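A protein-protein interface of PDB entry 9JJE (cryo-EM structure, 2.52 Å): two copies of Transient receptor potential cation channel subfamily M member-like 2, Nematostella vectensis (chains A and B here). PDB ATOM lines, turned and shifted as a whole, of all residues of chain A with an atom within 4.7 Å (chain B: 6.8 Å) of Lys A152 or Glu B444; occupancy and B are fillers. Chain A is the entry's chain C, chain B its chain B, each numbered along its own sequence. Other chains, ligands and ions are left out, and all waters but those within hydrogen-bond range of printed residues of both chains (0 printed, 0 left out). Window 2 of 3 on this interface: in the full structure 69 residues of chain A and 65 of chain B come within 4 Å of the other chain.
OE2 of Glu B444 sits at hydrogen-bond distance from OG of Ser A332. NH2 of Arg A154 lies close to NE2 of Gln B474 (3.0 Å). The side-chain carboxylate of Glu B444 lies close to the backbone carbonyl oxygen of Gly A326, at 3.3 Å.
The backbone carbonyl oxygen (O) of Lys A152 lies close to the guanidinium group (NE) of Arg A156 (3.3 Å). The backbone carbonyl oxygen (O) of Gly A328 sits at hydrogen-bond distance from the side-chain hydroxyl (OG) of Ser A332 (2.9 Å).
Among the printed residues, pairs that only touch across the chains: Val A150 with Gln B447 (3.98 Å), Lys A152 with Glu B444 (3.5 Å), Pro A153 with Asn B475 (3.3 Å) and Ser A327 with Glu B444 (3.6 Å).
Of chain B, only Glu B444 comes within 4 Å of Lys A152. Glu B444 touches four residues of chain A. Printed residues of chain A within 4 Å of Gln B447: Val A150. Printed residues of chain A within 4 Å of Gln B474: Arg A154. The nearest residue of chain B that does not touch Lys A152 is Thr B443 (4.4 Å). The nearest printed residue of chain B that does not touch Ser A327 is Glu B445 (8.6 Å).
Printed residues of chain B that touch a printed residue of chain A: Glu B444, Gln B447, Gln B474 and Asn B475. Hydrophobic or aromatic side chains of chain A within 4 Å of the printed part of chain B: Val A150 and Pro A153. Among the printed residues, no Asp or Glu carboxylate lies within 4 Å of a Lys or Arg side-chain nitrogen of the other chain.
No position is printed for both chains. Of the 7 pairs that touch across the chains among the printed residues, none has its exchanged pair printed and touching as well.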
ATOM      1  N   VAL A 150     -13.025 -30.735  -9.793  1.00  0.00           N
ATOM      2  CA  VAL A 150     -11.778 -29.998  -9.974  1.00  0.00           C
ATOM      3  C   VAL A 150     -10.749 -30.567  -9.007  1.00  0.00           C
ATOM      4  O   VAL A 150     -11.020 -30.683  -7.805  1.00  0.00           O
ATOM      5  CB  VAL A 150     -11.978 -28.489  -9.751  1.00  0.00           C
ATOM      6  CG1 VAL A 150     -10.656 -27.741  -9.871  1.00  0.00           C
ATOM      7  CG2 VAL A 150     -13.001 -27.937 -10.733  1.00  0.00           C
ATOM      8  N   LEU A 151      -9.572 -30.918  -9.528  1.00  0.00           N
ATOM      9  CA  LEU A 151      -8.593 -31.683  -8.769  1.00  0.00           C
ATOM     10  C   LEU A 151      -7.179 -31.196  -9.055  1.00  0.00           C
ATOM     11  O   LEU A 151      -6.849 -30.843 -10.191  1.00  0.00           O
ATOM     12  CB  LEU A 151      -8.716 -33.189  -9.076  1.00  0.00           C
ATOM     13  CG  LEU A 151      -8.315 -33.805 -10.422  1.00  0.00           C
ATOM     14  CD1 LEU A 151      -8.131 -35.297 -10.256  1.00  0.00           C
ATOM     15  CD2 LEU A 151      -9.318 -33.543 -11.554  1.00  0.00           C
ATOM     16  N   LYS A 152      -6.347 -31.173  -8.000  1.00  0.00           N
ATOM     17  CA  LYS A 152      -4.949 -30.756  -8.038  1.00  0.00           C
ATOM     18  C   LYS A 152      -4.060 -31.919  -8.486  1.00  0.00           C
ATOM     19  O   LYS A 152      -4.345 -33.072  -8.159  1.00  0.00           O
ATOM     20  CB  LYS A 152      -4.502 -30.265  -6.661  1.00  0.00           C
ATOM     21  CG  LYS A 152      -5.209 -29.012  -6.167  1.00  0.00           C
ATOM     22  CD  LYS A 152      -4.673 -28.584  -4.807  1.00  0.00           C
ATOM     23  CE  LYS A 152      -5.435 -27.386  -4.260  1.00  0.00           C
ATOM     24  NZ  LYS A 152      -5.190 -26.158  -5.062  1.00  0.00           N
ATOM     25  N   PRO A 153      -2.977 -31.647  -9.228  1.00  0.00           N
ATOM     26  CA  PRO A 153      -2.129 -32.758  -9.705  1.00  0.00           C
ATOM     27  C   PRO A 153      -1.314 -33.431  -8.610  1.00  0.00           C
ATOM     28  O   PRO A 153      -1.192 -34.666  -8.612  1.00  0.00           O
ATOM     29  CB  PRO A 153      -1.236 -32.086 -10.758  1.00  0.00           C
ATOM     30  CG  PRO A 153      -1.196 -30.653 -10.362  1.00  0.00           C
ATOM     31  CD  PRO A 153      -2.545 -30.348  -9.772  1.00  0.00           C
ATOM     32  N   ARG A 154      -0.748 -32.653  -7.679  1.00  0.00           N
ATOM     33  CA  ARG A 154      -0.062 -33.239  -6.530  1.00  0.00           C
ATOM     34  C   ARG A 154      -1.026 -34.047  -5.674  1.00  0.00           C
ATOM     35  O   ARG A 154      -0.706 -35.165  -5.246  1.00  0.00           O
ATOM     36  CB  ARG A 154       0.588 -32.147  -5.678  1.00  0.00           C
ATOM     37  CG  ARG A 154       1.398 -32.693  -4.501  1.00  0.00           C
ATOM     38  CD  ARG A 154       1.896 -31.607  -3.560  1.00  0.00           C
ATOM     39  NE  ARG A 154       2.879 -30.701  -4.150  1.00  0.00           N
ATOM     40  CZ  ARG A 154       3.325 -29.612  -3.534  1.00  0.00           C
ATOM     41  NH1 ARG A 154       2.882 -29.309  -2.325  1.00  0.00           N
ATOM     42  NH2 ARG A 154       4.216 -28.821  -4.113  1.00  0.00           N
ATOM     43  N   LEU A 155      -2.220 -33.500  -5.437  1.00  0.00           N
ATOM     44  CA  LEU A 155      -3.208 -34.179  -4.609  1.00  0.00           C
ATOM     45  C   LEU A 155      -3.740 -35.430  -5.296  1.00  0.00           C
ATOM     46  O   LEU A 155      -3.929 -36.458  -4.636  1.00  0.00           O
ATOM     47  CB  LEU A 155      -4.343 -33.216  -4.257  1.00  0.00           C
ATOM     48  CG  LEU A 155      -5.408 -33.619  -3.233  1.00  0.00           C
ATOM     49  CD1 LEU A 155      -5.777 -32.394  -2.439  1.00  0.00           C
ATOM     50  CD2 LEU A 155      -6.663 -34.179  -3.894  1.00  0.00           C
ATOM     51  N   ARG A 156      -3.958 -35.373  -6.619  1.00  0.00           N
ATOM     52  CA  ARG A 156      -4.443 -36.562  -7.318  1.00  0.00           C
ATOM     53  C   ARG A 156      -3.375 -37.647  -7.356  1.00  0.00           C
ATOM     54  O   ARG A 156      -3.704 -38.827  -7.196  1.00  0.00           O
ATOM     55  CB  ARG A 156      -4.941 -36.226  -8.740  1.00  0.00           C
ATOM     56  CG  ARG A 156      -3.885 -36.013  -9.835  1.00  0.00           C
ATOM     57  CD  ARG A 156      -4.424 -35.571 -11.194  1.00  0.00           C
ATOM     58  NE  ARG A 156      -4.837 -34.173 -11.223  1.00  0.00           N
ATOM     59  CZ  ARG A 156      -5.369 -33.576 -12.286  1.00  0.00           C
ATOM     60  NH1 ARG A 156      -5.560 -34.262 -13.405  1.00  0.00           N
ATOM     61  NH2 ARG A 156      -5.721 -32.299 -12.226  1.00  0.00           N
ATOM     62  N   GLU A 302     -13.659 -34.038  -2.708  1.00  0.00           N
ATOM     63  CA  GLU A 302     -14.065 -33.267  -3.890  1.00  0.00           C
ATOM     64  C   GLU A 302     -15.417 -33.724  -4.446  1.00  0.00           C
ATOM     65  O   GLU A 302     -15.529 -34.189  -5.581  1.00  0.00           O
ATOM     66  CB  GLU A 302     -12.977 -33.335  -4.967  1.00  0.00           C
ATOM     67  CG  GLU A 302     -11.648 -32.761  -4.520  1.00  0.00           C
ATOM     68  CD  GLU A 302     -10.567 -32.901  -5.565  1.00  0.00           C
ATOM     69  OE1 GLU A 302     -10.821 -33.566  -6.588  1.00  0.00           O
ATOM     70  OE2 GLU A 302      -9.467 -32.346  -5.363  1.00  0.00           O
ATOM     71  N   GLY A 326      -8.745 -29.837   2.441  1.00  0.00           N
ATOM     72  CA  GLY A 326      -7.892 -29.134   1.510  1.00  0.00           C
ATOM     73  C   GLY A 326      -7.914 -29.696   0.111  1.00  0.00           C
ATOM     74  O   GLY A 326      -6.955 -29.504  -0.641  1.00  0.00           O
ATOM     75  N   SER A 327      -8.984 -30.397  -0.261  1.00  0.00           N
ATOM     76  CA  SER A 327      -9.087 -31.029  -1.569  1.00  0.00           C
ATOM     77  C   SER A 327     -10.001 -30.276  -2.525  1.00  0.00           C
ATOM     78  O   SER A 327      -9.576 -29.904  -3.623  1.00  0.00           O
ATOM     79  CB  SER A 327      -9.571 -32.476  -1.417  1.00  0.00           C
ATOM     80  OG  SER A 327     -10.901 -32.521  -0.930  1.00  0.00           O
ATOM     81  N   GLY A 328     -11.251 -30.043  -2.136  1.00  0.00           N
ATOM     82  CA  GLY A 328     -12.205 -29.461  -3.056  1.00  0.00           C
ATOM     83  C   GLY A 328     -13.289 -28.614  -2.431  1.00  0.00           C
ATOM     84  O   GLY A 328     -13.024 -27.784  -1.556  1.00  0.00           O
ATOM     85  N   SER A 332     -13.689 -29.883   1.975  1.00  0.00           N
ATOM     86  CA  SER A 332     -13.198 -28.752   2.750  1.00  0.00           C
ATOM     87  C   SER A 332     -14.260 -28.228   3.708  1.00  0.00           C
ATOM     88  O   SER A 332     -13.923 -27.754   4.796  1.00  0.00           O
ATOM     89  CB  SER A 332     -12.731 -27.638   1.814  1.00  0.00           C
ATOM     90  OG  SER A 332     -11.632 -28.062   1.027  1.00  0.00           O
ATOM     91  N   SER B 439       4.133 -20.924   0.778  1.00  0.00           N
ATOM     92  CA  SER B 439       3.204 -20.587   1.851  1.00  0.00           C
ATOM     93  C   SER B 439       2.033 -19.747   1.352  1.00  0.00           C
ATOM     94  O   SER B 439       0.870 -20.126   1.521  1.00  0.00           O
ATOM     95  CB  SER B 439       3.948 -19.857   2.971  1.00  0.00           C
ATOM     96  OG  SER B 439       4.923 -20.695   3.567  1.00  0.00           O
ATOM     97  N   PHE B 442       1.069 -20.030  -3.501  1.00  0.00           N
ATOM     98  CA  PHE B 442       0.517 -21.257  -4.062  1.00  0.00           C
ATOM     99  C   PHE B 442      -0.502 -21.889  -3.121  1.00  0.00           C
ATOM    100  O   PHE B 442      -0.510 -23.103  -2.907  1.00  0.00           O
ATOM    101  CB  PHE B 442       1.629 -22.245  -4.402  1.00  0.00           C
ATOM    102  CG  PHE B 442       2.403 -21.871  -5.629  1.00  0.00           C
ATOM    103  CD1 PHE B 442       1.939 -22.226  -6.884  1.00  0.00           C
ATOM    104  CD2 PHE B 442       3.576 -21.140  -5.533  1.00  0.00           C
ATOM    105  CE1 PHE B 442       2.639 -21.875  -8.021  1.00  0.00           C
ATOM    106  CE2 PHE B 442       4.279 -20.786  -6.663  1.00  0.00           C
ATOM    107  CZ  PHE B 442       3.808 -21.154  -7.909  1.00  0.00           C
ATOM    108  N   THR B 443      -1.360 -21.055  -2.534  1.00  0.00           N
ATOM    109  CA  THR B 443      -2.400 -21.513  -1.626  1.00  0.00           C
ATOM    110  C   THR B 443      -3.479 -22.301  -2.376  1.00  0.00           C
ATOM    111  O   THR B 443      -3.489 -22.403  -3.607  1.00  0.00           O
ATOM    112  CB  THR B 443      -3.037 -20.329  -0.898  1.00  0.00           C
ATOM    113  OG1 THR B 443      -3.663 -19.460  -1.850  1.00  0.00           O
ATOM    114  CG2 THR B 443      -1.986 -19.549  -0.127  1.00  0.00           C
ATOM    115  N   GLU B 444      -4.408 -22.858  -1.596  1.00  0.00           N
ATOM    116  CA  GLU B 444      -5.457 -23.706  -2.156  1.00  0.00           C
ATOM    117  C   GLU B 444      -6.489 -22.892  -2.928  1.00  0.00           C
ATOM    118  O   GLU B 444      -6.889 -23.270  -4.036  1.00  0.00           O
ATOM    119  CB  GLU B 444      -6.136 -24.497  -1.038  1.00  0.00           C
ATOM    120  CG  GLU B 444      -7.253 -25.395  -1.524  1.00  0.00           C
ATOM    121  CD  GLU B 444      -7.951 -26.116  -0.397  1.00  0.00           C
ATOM    122  OE1 GLU B 444      -7.543 -25.931   0.770  1.00  0.00           O
ATOM    123  OE2 GLU B 444      -8.922 -26.848  -0.676  1.00  0.00           O
ATOM    124  N   GLU B 445      -6.939 -21.773  -2.350  1.00  0.00           N
ATOM    125  CA  GLU B 445      -8.048 -21.007  -2.915  1.00  0.00           C
ATOM    126  C   GLU B 445      -7.691 -20.308  -4.220  1.00  0.00           C
ATOM    127  O   GLU B 445      -8.597 -19.922  -4.968  1.00  0.00           O
ATOM    128  CB  GLU B 445      -8.541 -19.978  -1.894  1.00  0.00           C
ATOM    129  CG  GLU B 445      -7.517 -18.909  -1.549  1.00  0.00           C
ATOM    130  CD  GLU B 445      -8.009 -17.951  -0.483  1.00  0.00           C
ATOM    131  OE1 GLU B 445      -9.144 -18.136   0.006  1.00  0.00           O
ATOM    132  OE2 GLU B 445      -7.260 -17.015  -0.133  1.00  0.00           O
ATOM    133  N   GLN B 446      -6.407 -20.133  -4.512  1.00  0.00           N
ATOM    134  CA  GLN B 446      -5.956 -19.514  -5.750  1.00  0.00           C
ATOM    135  C   GLN B 446      -5.427 -20.605  -6.675  1.00  0.00           C
ATOM    136  O   GLN B 446      -4.476 -21.313  -6.327  1.00  0.00           O
ATOM    137  CB  GLN B 446      -4.892 -18.455  -5.459  1.00  0.00           C
ATOM    138  CG  GLN B 446      -4.473 -17.606  -6.649  1.00  0.00           C
ATOM    139  CD  GLN B 446      -3.281 -18.187  -7.373  1.00  0.00           C
ATOM    140  OE1 GLN B 446      -2.455 -18.867  -6.767  1.00  0.00           O
ATOM    141  NE2 GLN B 446      -3.186 -17.929  -8.673  1.00  0.00           N
ATOM    142  N   GLN B 447      -6.041 -20.733  -7.849  1.00  0.00           N
ATOM    143  CA  GLN B 447      -5.745 -21.809  -8.787  1.00  0.00           C
ATOM    144  C   GLN B 447      -4.849 -21.296  -9.907  1.00  0.00           C
ATOM    145  O   GLN B 447      -5.106 -20.229 -10.475  1.00  0.00           O
ATOM    146  CB  GLN B 447      -7.040 -22.384  -9.367  1.00  0.00           C
ATOM    147  CG  GLN B 447      -6.843 -23.581 -10.284  1.00  0.00           C
ATOM    148  CD  GLN B 447      -8.155 -24.153 -10.789  1.00  0.00           C
ATOM    149  OE1 GLN B 447      -9.230 -23.633 -10.486  1.00  0.00           O
ATOM    150  NE2 GLN B 447      -8.073 -25.230 -11.559  1.00  0.00           N
ATOM    151  N   TRP B 448      -3.803 -22.056 -10.219  1.00  0.00           N
ATOM    152  CA  TRP B 448      -2.869 -21.721 -11.283  1.00  0.00           C
ATOM    153  C   TRP B 448      -3.147 -22.551 -12.531  1.00  0.00           C
ATOM    154  O   TRP B 448      -3.747 -23.627 -12.475  1.00  0.00           O
ATOM    155  CB  TRP B 448      -1.423 -21.943 -10.832  1.00  0.00           C
ATOM    156  CG  TRP B 448      -0.953 -20.978  -9.797  1.00  0.00           C
ATOM    157  CD1 TRP B 448      -0.897 -21.185  -8.451  1.00  0.00           C
ATOM    158  CD2 TRP B 448      -0.466 -19.649 -10.019  1.00  0.00           C
ATOM    159  NE1 TRP B 448      -0.404 -20.069  -7.820  1.00  0.00           N
ATOM    160  CE2 TRP B 448      -0.129 -19.112  -8.762  1.00  0.00           C
ATOM    161  CE3 TRP B 448      -0.282 -18.861 -11.159  1.00  0.00           C
ATOM    162  CZ2 TRP B 448       0.375 -17.823  -8.610  1.00  0.00           C
ATOM    163  CZ3 TRP B 448       0.224 -17.582 -11.009  1.00  0.00           C
ATOM    164  CH2 TRP B 448       0.544 -17.076  -9.743  1.00  0.00           C
ATOM    165  N   GLN B 474       4.505 -29.126 -10.294  1.00  0.00           N
ATOM    166  CA  GLN B 474       3.640 -29.876  -9.387  1.00  0.00           C
ATOM    167  C   GLN B 474       2.521 -29.039  -8.763  1.00  0.00           C
ATOM    168  O   GLN B 474       1.867 -29.512  -7.827  1.00  0.00           O
ATOM    169  CB  GLN B 474       4.467 -30.570  -8.293  1.00  0.00           C
ATOM    170  CG  GLN B 474       5.114 -29.687  -7.239  1.00  0.00           C
ATOM    171  CD  GLN B 474       6.047 -30.475  -6.330  1.00  0.00           C
ATOM    172  OE1 GLN B 474       6.148 -31.698  -6.437  1.00  0.00           O
ATOM    173  NE2 GLN B 474       6.750 -29.775  -5.447  1.00  0.00           N
ATOM    174  N   ASN B 475       2.264 -27.825  -9.258  1.00  0.00           N
ATOM    175  CA  ASN B 475       1.047 -27.106  -8.878  1.00  0.00           C
ATOM    176  C   ASN B 475       0.025 -26.974  -9.999  1.00  0.00           C
ATOM    177  O   ASN B 475      -1.120 -27.402  -9.832  1.00  0.00           O
ATOM    178  CB  ASN B 475       1.368 -25.708  -8.326  1.00  0.00           C
ATOM    179  CG  ASN B 475       1.849 -25.742  -6.890  1.00  0.00           C
ATOM    180  OD1 ASN B 475       2.961 -25.321  -6.583  1.00  0.00           O
ATOM    181  ND2 ASN B 475       1.001 -26.244  -5.999  1.00  0.00           N
